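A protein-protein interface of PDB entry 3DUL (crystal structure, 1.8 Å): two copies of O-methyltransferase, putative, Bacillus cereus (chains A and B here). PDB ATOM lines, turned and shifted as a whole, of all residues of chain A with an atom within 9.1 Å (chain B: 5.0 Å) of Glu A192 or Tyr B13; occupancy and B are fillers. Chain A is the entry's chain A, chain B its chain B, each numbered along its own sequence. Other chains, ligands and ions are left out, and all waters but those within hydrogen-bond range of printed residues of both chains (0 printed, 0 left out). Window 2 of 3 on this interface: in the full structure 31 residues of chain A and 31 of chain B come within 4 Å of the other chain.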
ATOM      1  N   PHE A 150      -7.151 -14.483 -11.995  1.00  0.00           N
ATOM      2  CA  PHE A 150      -8.017 -14.553 -10.825  1.00  0.00           C
ATOM      3  C   PHE A 150      -7.286 -15.310  -9.719  1.00  0.00           C
ATOM      4  O   PHE A 150      -7.272 -14.880  -8.568  1.00  0.00           O
ATOM      5  CB  PHE A 150      -9.325 -15.277 -11.147  1.00  0.00           C
ATOM      6  CG  PHE A 150     -10.117 -15.646  -9.923  1.00  0.00           C
ATOM      7  CD1 PHE A 150     -10.794 -14.674  -9.200  1.00  0.00           C
ATOM      8  CD2 PHE A 150     -10.133 -16.958  -9.460  1.00  0.00           C
ATOM      9  CE1 PHE A 150     -11.476 -14.997  -8.028  1.00  0.00           C
ATOM     10  CE2 PHE A 150     -10.811 -17.294  -8.289  1.00  0.00           C
ATOM     11  CZ  PHE A 150     -11.484 -16.306  -7.572  1.00  0.00           C
ATOM     12  N   GLU A 151      -6.686 -16.445 -10.068  1.00  0.00           N
ATOM     13  CA  GLU A 151      -5.954 -17.228  -9.076  1.00  0.00           C
ATOM     14  C   GLU A 151      -4.785 -16.420  -8.528  1.00  0.00           C
ATOM     15  O   GLU A 151      -4.479 -16.484  -7.338  1.00  0.00           O
ATOM     16  CB  GLU A 151      -5.468 -18.548  -9.684  1.00  0.00           C
ATOM     17  CG  GLU A 151      -6.571 -19.590  -9.843  1.00  0.00           C
ATOM     18  CD  GLU A 151      -7.299 -19.873  -8.539  1.00  0.00           C
ATOM     19  OE1 GLU A 151      -6.625 -20.095  -7.508  1.00  0.00           O
ATOM     20  OE2 GLU A 151      -8.548 -19.875  -8.539  1.00  0.00           O
ATOM     21  N   ASN A 167     -15.431  -9.428 -17.629  1.00  0.00           N
ATOM     22  CA  ASN A 167     -15.609 -10.652 -18.380  1.00  0.00           C
ATOM     23  C   ASN A 167     -15.760 -10.351 -19.856  1.00  0.00           C
ATOM     24  O   ASN A 167     -14.782 -10.355 -20.596  1.00  0.00           O
ATOM     25  CB  ASN A 167     -16.820 -11.431 -17.887  1.00  0.00           C
ATOM     26  CG  ASN A 167     -16.468 -12.847 -17.519  1.00  0.00           C
ATOM     27  OD1 ASN A 167     -16.029 -13.116 -16.397  1.00  0.00           O
ATOM     28  ND2 ASN A 167     -16.627 -13.765 -18.469  1.00  0.00           N
ATOM     29  N   ILE A 187     -16.530 -18.604 -20.492  1.00  0.00           N
ATOM     30  CA  ILE A 187     -17.482 -17.751 -19.796  1.00  0.00           C
ATOM     31  C   ILE A 187     -18.132 -18.542 -18.664  1.00  0.00           C
ATOM     32  O   ILE A 187     -17.972 -18.208 -17.492  1.00  0.00           O
ATOM     33  CB  ILE A 187     -18.581 -17.243 -20.756  1.00  0.00           C
ATOM     34  CG1 ILE A 187     -17.941 -16.699 -22.042  1.00  0.00           C
ATOM     35  CG2 ILE A 187     -19.399 -16.163 -20.064  1.00  0.00           C
ATOM     36  CD1 ILE A 187     -18.933 -16.302 -23.121  1.00  0.00           C
ATOM     37  N   ARG A 188     -18.860 -19.598 -19.013  1.00  0.00           N
ATOM     38  CA  ARG A 188     -19.504 -20.423 -17.998  1.00  0.00           C
ATOM     39  C   ARG A 188     -18.435 -21.090 -17.139  1.00  0.00           C
ATOM     40  O   ARG A 188     -18.592 -21.228 -15.927  1.00  0.00           O
ATOM     41  CB  ARG A 188     -20.374 -21.505 -18.642  1.00  0.00           C
ATOM     42  CG  ARG A 188     -21.485 -20.985 -19.538  1.00  0.00           C
ATOM     43  CD  ARG A 188     -22.380 -22.133 -19.982  1.00  0.00           C
ATOM     44  NE  ARG A 188     -23.251 -21.762 -21.095  1.00  0.00           N
ATOM     45  CZ  ARG A 188     -24.136 -22.582 -21.653  1.00  0.00           C
ATOM     46  NH1 ARG A 188     -24.268 -23.823 -21.200  1.00  0.00           N
ATOM     47  NH2 ARG A 188     -24.882 -22.166 -22.671  1.00  0.00           N
ATOM     48  N   ARG A 189     -17.339 -21.497 -17.771  1.00  0.00           N
ATOM     49  CA  ARG A 189     -16.268 -22.158 -17.041  1.00  0.00           C
ATOM     50  C   ARG A 189     -15.516 -21.229 -16.092  1.00  0.00           C
ATOM     51  O   ARG A 189     -15.037 -21.671 -15.047  1.00  0.00           O
ATOM     52  CB  ARG A 189     -15.308 -22.831 -18.026  1.00  0.00           C
ATOM     53  CG  ARG A 189     -15.976 -23.981 -18.772  1.00  0.00           C
ATOM     54  CD  ARG A 189     -15.010 -24.773 -19.631  1.00  0.00           C
ATOM     55  NE  ARG A 189     -15.665 -25.939 -20.220  1.00  0.00           N
ATOM     56  CZ  ARG A 189     -16.236 -26.915 -19.515  1.00  0.00           C
ATOM     57  NH1 ARG A 189     -16.235 -26.875 -18.188  1.00  0.00           N
ATOM     58  NH2 ARG A 189     -16.812 -27.934 -20.140  1.00  0.00           N
ATOM     59  N   PHE A 190     -15.418 -19.950 -16.446  1.00  0.00           N
ATOM     60  CA  PHE A 190     -14.732 -18.988 -15.588  1.00  0.00           C
ATOM     61  C   PHE A 190     -15.539 -18.737 -14.314  1.00  0.00           C
ATOM     62  O   PHE A 190     -14.976 -18.483 -13.247  1.00  0.00           O
ATOM     63  CB  PHE A 190     -14.504 -17.670 -16.336  1.00  0.00           C
ATOM     64  CG  PHE A 190     -13.849 -16.599 -15.501  1.00  0.00           C
ATOM     65  CD1 PHE A 190     -12.852 -16.917 -14.582  1.00  0.00           C
ATOM     66  CD2 PHE A 190     -14.226 -15.269 -15.637  1.00  0.00           C
ATOM     67  CE1 PHE A 190     -12.242 -15.929 -13.814  1.00  0.00           C
ATOM     68  CE2 PHE A 190     -13.622 -14.272 -14.874  1.00  0.00           C
ATOM     69  CZ  PHE A 190     -12.627 -14.605 -13.959  1.00  0.00           C
ATOM     70  N   TYR A 191     -16.861 -18.810 -14.426  1.00  0.00           N
ATOM     71  CA  TYR A 191     -17.720 -18.603 -13.268  1.00  0.00           C
ATOM     72  C   TYR A 191     -17.810 -19.895 -12.465  1.00  0.00           C
ATOM     73  O   TYR A 191     -17.981 -19.864 -11.249  1.00  0.00           O
ATOM     74  CB  TYR A 191     -19.110 -18.150 -13.712  1.00  0.00           C
ATOM     75  CG  TYR A 191     -19.150 -16.712 -14.177  1.00  0.00           C
ATOM     76  CD1 TYR A 191     -18.935 -15.668 -13.282  1.00  0.00           C
ATOM     77  CD2 TYR A 191     -19.395 -16.396 -15.511  1.00  0.00           C
ATOM     78  CE1 TYR A 191     -18.965 -14.339 -13.702  1.00  0.00           C
ATOM     79  CE2 TYR A 191     -19.427 -15.072 -15.944  1.00  0.00           C
ATOM     80  CZ  TYR A 191     -19.211 -14.050 -15.032  1.00  0.00           C
ATOM     81  OH  TYR A 191     -19.253 -12.742 -15.456  1.00  0.00           O
ATOM     82  N   GLU A 192     -17.700 -21.029 -13.154  1.00  0.00           N
ATOM     83  CA  GLU A 192     -17.731 -22.323 -12.483  1.00  0.00           C
ATOM     84  C   GLU A 192     -16.459 -22.393 -11.647  1.00  0.00           C
ATOM     85  O   GLU A 192     -16.444 -22.954 -10.551  1.00  0.00           O
ATOM     86  CB  GLU A 192     -17.733 -23.467 -13.500  1.00  0.00           C
ATOM     87  CG  GLU A 192     -18.995 -23.578 -14.337  1.00  0.00           C
ATOM     88  CD  GLU A 192     -18.914 -24.705 -15.351  1.00  0.00           C
ATOM     89  OE1 GLU A 192     -18.685 -25.863 -14.940  1.00  0.00           O
ATOM     90  OE2 GLU A 192     -19.078 -24.436 -16.560  1.00  0.00           O
ATOM     91  N   LEU A 193     -15.392 -21.822 -12.194  1.00  0.00           N
ATOM     92  CA  LEU A 193     -14.101 -21.779 -11.518  1.00  0.00           C
ATOM     93  C   LEU A 193     -14.307 -21.022 -10.216  1.00  0.00           C
ATOM     94  O   LEU A 193     -14.009 -21.526  -9.132  1.00  0.00           O
ATOM     95  CB  LEU A 193     -13.078 -21.047 -12.398  1.00  0.00           C
ATOM     96  CG  LEU A 193     -11.659 -20.765 -11.886  1.00  0.00           C
ATOM     97  CD1 LEU A 193     -10.868 -20.128 -13.010  1.00  0.00           C
ATOM     98  CD2 LEU A 193     -11.670 -19.845 -10.687  1.00  0.00           C
ATOM     99  N   ILE A 194     -14.823 -19.800 -10.334  1.00  0.00           N
ATOM    100  CA  ILE A 194     -15.078 -18.957  -9.171  1.00  0.00           C
ATOM    101  C   ILE A 194     -16.006 -19.677  -8.209  1.00  0.00           C
ATOM    102  O   ILE A 194     -15.752 -19.735  -7.007  1.00  0.00           O
ATOM    103  CB  ILE A 194     -15.753 -17.632  -9.575  1.00  0.00           C
ATOM    104  CG1 ILE A 194     -14.926 -16.929 -10.652  1.00  0.00           C
ATOM    105  CG2 ILE A 194     -15.912 -16.742  -8.356  1.00  0.00           C
ATOM    106  CD1 ILE A 194     -13.526 -16.585 -10.217  1.00  0.00           C
ATOM    107  N   ALA A 195     -17.086 -20.228  -8.753  1.00  0.00           N
ATOM    108  CA  ALA A 195     -18.057 -20.958  -7.956  1.00  0.00           C
ATOM    109  C   ALA A 195     -17.371 -22.125  -7.256  1.00  0.00           C
ATOM    110  O   ALA A 195     -17.813 -22.574  -6.198  1.00  0.00           O
ATOM    111  CB  ALA A 195     -19.187 -21.466  -8.852  1.00  0.00           C
ATOM    112  N   ALA A 196     -16.279 -22.605  -7.847  1.00  0.00           N
ATOM    113  CA  ALA A 196     -15.526 -23.722  -7.286  1.00  0.00           C
ATOM    114  C   ALA A 196     -14.350 -23.248  -6.435  1.00  0.00           C
ATOM    115  O   ALA A 196     -13.459 -24.033  -6.097  1.00  0.00           O
ATOM    116  CB  ALA A 196     -15.028 -24.621  -8.403  1.00  0.00           C
ATOM    117  N   GLU A 197     -14.345 -21.960  -6.101  1.00  0.00           N
ATOM    118  CA  GLU A 197     -13.288 -21.385  -5.280  1.00  0.00           C
ATOM    119  C   GLU A 197     -13.886 -20.910  -3.960  1.00  0.00           C
ATOM    120  O   GLU A 197     -14.401 -19.794  -3.862  1.00  0.00           O
ATOM    121  CB  GLU A 197     -12.613 -20.224  -6.017  1.00  0.00           C
ATOM    122  CG  GLU A 197     -11.542 -19.526  -5.201  1.00  0.00           C
ATOM    123  CD  GLU A 197     -10.519 -20.490  -4.637  1.00  0.00           C
ATOM    124  OE1 GLU A 197      -9.665 -20.990  -5.404  1.00  0.00           O
ATOM    125  OE2 GLU A 197     -10.578 -20.754  -3.422  1.00  0.00           O
ATOM    126  N   PRO A 198     -13.832 -21.767  -2.925  1.00  0.00           N
ATOM    127  CA  PRO A 198     -14.348 -21.518  -1.574  1.00  0.00           C
ATOM    128  C   PRO A 198     -13.725 -20.330  -0.855  1.00  0.00           C
ATOM    129  O   PRO A 198     -14.298 -19.815   0.101  1.00  0.00           O
ATOM    130  CB  PRO A 198     -14.054 -22.830  -0.842  1.00  0.00           C
ATOM    131  CG  PRO A 198     -14.071 -23.848  -1.945  1.00  0.00           C
ATOM    132  CD  PRO A 198     -13.309 -23.142  -3.029  1.00  0.00           C
ATOM    133  N   ALA A 204     -22.335 -11.296  -9.883  1.00  0.00           N
ATOM    134  CA  ALA A 204     -22.061 -10.779 -11.210  1.00  0.00           C
ATOM    135  C   ALA A 204     -23.048  -9.685 -11.564  1.00  0.00           C
ATOM    136  O   ALA A 204     -24.224  -9.750 -11.207  1.00  0.00           O
ATOM    137  CB  ALA A 204     -22.139 -11.893 -12.236  1.00  0.00           C
ATOM    138  N   ILE A 217     -17.472  -9.672 -12.635  1.00  0.00           N
ATOM    139  CA  ILE A 217     -17.715 -10.342 -11.370  1.00  0.00           C
ATOM    140  C   ILE A 217     -17.186  -9.456 -10.249  1.00  0.00           C
ATOM    141  O   ILE A 217     -16.219  -8.718 -10.433  1.00  0.00           O
ATOM    142  CB  ILE A 217     -17.011 -11.714 -11.336  1.00  0.00           C
ATOM    143  CG1 ILE A 217     -17.370 -12.462 -10.051  1.00  0.00           C
ATOM    144  CG2 ILE A 217     -15.513 -11.521 -11.421  1.00  0.00           C
ATOM    145  CD1 ILE A 217     -16.962 -13.918 -10.069  1.00  0.00           C
ATOM    146  N   THR B   8     -29.546 -13.281 -21.342  1.00  0.00           N
ATOM    147  CA  THR B   8     -30.295 -13.401 -20.106  1.00  0.00           C
ATOM    148  C   THR B   8     -30.128 -14.835 -19.610  1.00  0.00           C
ATOM    149  O   THR B   8     -29.882 -15.072 -18.428  1.00  0.00           O
ATOM    150  CB  THR B   8     -31.786 -13.096 -20.328  1.00  0.00           C
ATOM    151  OG1 THR B   8     -31.928 -11.771 -20.862  1.00  0.00           O
ATOM    152  CG2 THR B   8     -32.544 -13.189 -19.015  1.00  0.00           C
ATOM    153  N   ALA B   9     -30.236 -15.788 -20.530  1.00  0.00           N
ATOM    154  CA  ALA B   9     -30.104 -17.200 -20.191  1.00  0.00           C
ATOM    155  C   ALA B   9     -28.725 -17.469 -19.619  1.00  0.00           C
ATOM    156  O   ALA B   9     -28.576 -18.179 -18.624  1.00  0.00           O
ATOM    157  CB  ALA B   9     -30.336 -18.058 -21.428  1.00  0.00           C
ATOM    158  N   VAL B  10     -27.712 -16.900 -20.259  1.00  0.00           N
ATOM    159  CA  VAL B  10     -26.344 -17.081 -19.797  1.00  0.00           C
ATOM    160  C   VAL B  10     -26.143 -16.498 -18.401  1.00  0.00           C
ATOM    161  O   VAL B  10     -25.535 -17.130 -17.542  1.00  0.00           O
ATOM    162  CB  VAL B  10     -25.340 -16.422 -20.758  1.00  0.00           C
ATOM    163  CG1 VAL B  10     -23.931 -16.519 -20.177  1.00  0.00           C
ATOM    164  CG2 VAL B  10     -25.402 -17.098 -22.122  1.00  0.00           C
ATOM    165  N   ASP B  11     -26.668 -15.300 -18.163  1.00  0.00           N
ATOM    166  CA  ASP B  11     -26.499 -14.674 -16.861  1.00  0.00           C
ATOM    167  C   ASP B  11     -27.296 -15.329 -15.746  1.00  0.00           C
ATOM    168  O   ASP B  11     -26.907 -15.266 -14.583  1.00  0.00           O
ATOM    169  CB  ASP B  11     -26.823 -13.187 -16.939  1.00  0.00           C
ATOM    170  CG  ASP B  11     -25.848 -12.441 -17.820  1.00  0.00           C
ATOM    171  OD1 ASP B  11     -24.682 -12.888 -17.902  1.00  0.00           O
ATOM    172  OD2 ASP B  11     -26.236 -11.419 -18.420  1.00  0.00           O
ATOM    173  N   GLN B  12     -28.413 -15.959 -16.087  1.00  0.00           N
ATOM    174  CA  GLN B  12     -29.198 -16.622 -15.062  1.00  0.00           C
ATOM    175  C   GLN B  12     -28.483 -17.909 -14.691  1.00  0.00           C
ATOM    176  O   GLN B  12     -28.545 -18.354 -13.546  1.00  0.00           O
ATOM    177  CB  GLN B  12     -30.616 -16.881 -15.568  1.00  0.00           C
ATOM    178  CG  GLN B  12     -31.399 -15.588 -15.711  1.00  0.00           C
ATOM    179  CD  GLN B  12     -32.720 -15.772 -16.412  1.00  0.00           C
ATOM    180  OE1 GLN B  12     -32.789 -16.399 -17.472  1.00  0.00           O
ATOM    181  NE2 GLN B  12     -33.779 -15.215 -15.836  1.00  0.00           N
ATOM    182  N   TYR B  13     -27.787 -18.497 -15.660  1.00  0.00           N
ATOM    183  CA  TYR B  13     -27.023 -19.711 -15.407  1.00  0.00           C
ATOM    184  C   TYR B  13     -25.890 -19.330 -14.451  1.00  0.00           C
ATOM    185  O   TYR B  13     -25.607 -20.032 -13.478  1.00  0.00           O
ATOM    186  CB  TYR B  13     -26.430 -20.255 -16.709  1.00  0.00           C
ATOM    187  CG  TYR B  13     -25.388 -21.332 -16.487  1.00  0.00           C
ATOM    188  CD1 TYR B  13     -25.757 -22.615 -16.081  1.00  0.00           C
ATOM    189  CD2 TYR B  13     -24.026 -21.048 -16.618  1.00  0.00           C
ATOM    190  CE1 TYR B  13     -24.795 -23.590 -15.803  1.00  0.00           C
ATOM    191  CE2 TYR B  13     -23.055 -22.016 -16.341  1.00  0.00           C
ATOM    192  CZ  TYR B  13     -23.447 -23.282 -15.933  1.00  0.00           C
ATOM    193  OH  TYR B  13     -22.491 -24.228 -15.627  1.00  0.00           O
ATOM    194  N   VAL B  14     -25.245 -18.205 -14.748  1.00  0.00           N
ATOM    195  CA  VAL B  14     -24.144 -17.695 -13.932  1.00  0.00           C
ATOM    196  C   VAL B  14     -24.625 -17.446 -12.509  1.00  0.00           C
ATOM    197  O   VAL B  14     -23.931 -17.766 -11.544  1.00  0.00           O
ATOM    198  CB  VAL B  14     -23.590 -16.374 -14.520  1.00  0.00           C
ATOM    199  CG1 VAL B  14     -22.624 -15.716 -13.533  1.00  0.00           C
ATOM    200  CG2 VAL B  14     -22.892 -16.659 -15.836  1.00  0.00           C
ATOM    201  N   SER B  15     -25.817 -16.868 -12.384  1.00  0.00           N
ATOM    202  CA  SER B  15     -26.378 -16.596 -11.070  1.00  0.00           C
ATOM    203  C   SER B  15     -26.545 -17.909 -10.321  1.00  0.00           C
ATOM    204  O   SER B  15     -26.324 -17.983  -9.111  1.00  0.00           O
ATOM    205  CB  SER B  15     -27.737 -15.912 -11.192  1.00  0.00           C
ATOM    206  OG  SER B  15     -28.304 -15.728  -9.906  1.00  0.00           O
ATOM    207  N   ASP B  16     -26.923 -18.945 -11.057  1.00  0.00           N
ATOM    208  CA  ASP B  16     -27.133 -20.266 -10.476  1.00  0.00           C
ATOM    209  C   ASP B  16     -25.859 -20.932  -9.974  1.00  0.00           C
ATOM    210  O   ASP B  16     -25.885 -21.631  -8.962  1.00  0.00           O
ATOM    211  CB  ASP B  16     -27.817 -21.188 -11.487  1.00  0.00           C
ATOM    212  CG  ASP B  16     -29.307 -20.930 -11.600  1.00  0.00           C
ATOM    213  OD1 ASP B  16     -29.813 -20.030 -10.894  1.00  0.00           O
ATOM    214  OD2 ASP B  16     -29.973 -21.632 -12.393  1.00  0.00           O
ATOM    215  N   VAL B  17     -24.745 -20.728 -10.669  1.00  0.00           N
ATOM    216  CA  VAL B  17     -23.498 -21.355 -10.243  1.00  0.00           C
ATOM    217  C   VAL B  17     -22.757 -20.535  -9.190  1.00  0.00           C
ATOM    218  O   VAL B  17     -22.223 -21.091  -8.229  1.00  0.00           O
ATOM    219  CB  VAL B  17     -22.555 -21.620 -11.442  1.00  0.00           C
ATOM    220  CG1 VAL B  17     -23.330 -22.280 -12.562  1.00  0.00           C
ATOM    221  CG2 VAL B  17     -21.912 -20.337 -11.912  1.00  0.00           C
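The side-chain hydroxyl of Tyr A191 is in hydrogen-bond range of the side-chain amide oxygen of Asn A167 (3.4 Å).
Printed residues of chain B within 4 Å of Tyr A191: Val B14 and Val B17. Glu A192 touches one residue of chain B. Printed residues of chain B within 4 Å of Ala A195: Val B17 (3.1 Å). Ile A217 touches none of the printed residues of chain B. Tyr B13 touches two residues of chain A. Val B14 touches just one residue of chain A: Tyr A191 (3.5 Å). Printed residues of chain A within 4 Å of Val B17: Tyr A191 and Ala A195. The nearest residue of chain B that does not touch Glu A192 is Val B17 (4.4 Å).
Tyr B13 touches Arg A188 (CE2 to CB, 3.6 Å). Val B14 touches Tyr A191 (CG2 to CD2, 3.5 Å). Val B17 touches Tyr A191 (CG2 to CB, 3.98 Å). OH of Tyr B13 touches OE2 of Glu A192, 3.5 Å away. O of Val B17 touches CB of Ala A195, 3.1 Å away.
Printed residues of chain B that touch a printed residue of chain A: Tyr B13, Val B14 and Val B17. Hydrophobic or aromatic side chains of chain B within 4 Å of the printed part of chain A: Tyr B13, Val B14 and Val B17.
No position is printed for both chains.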
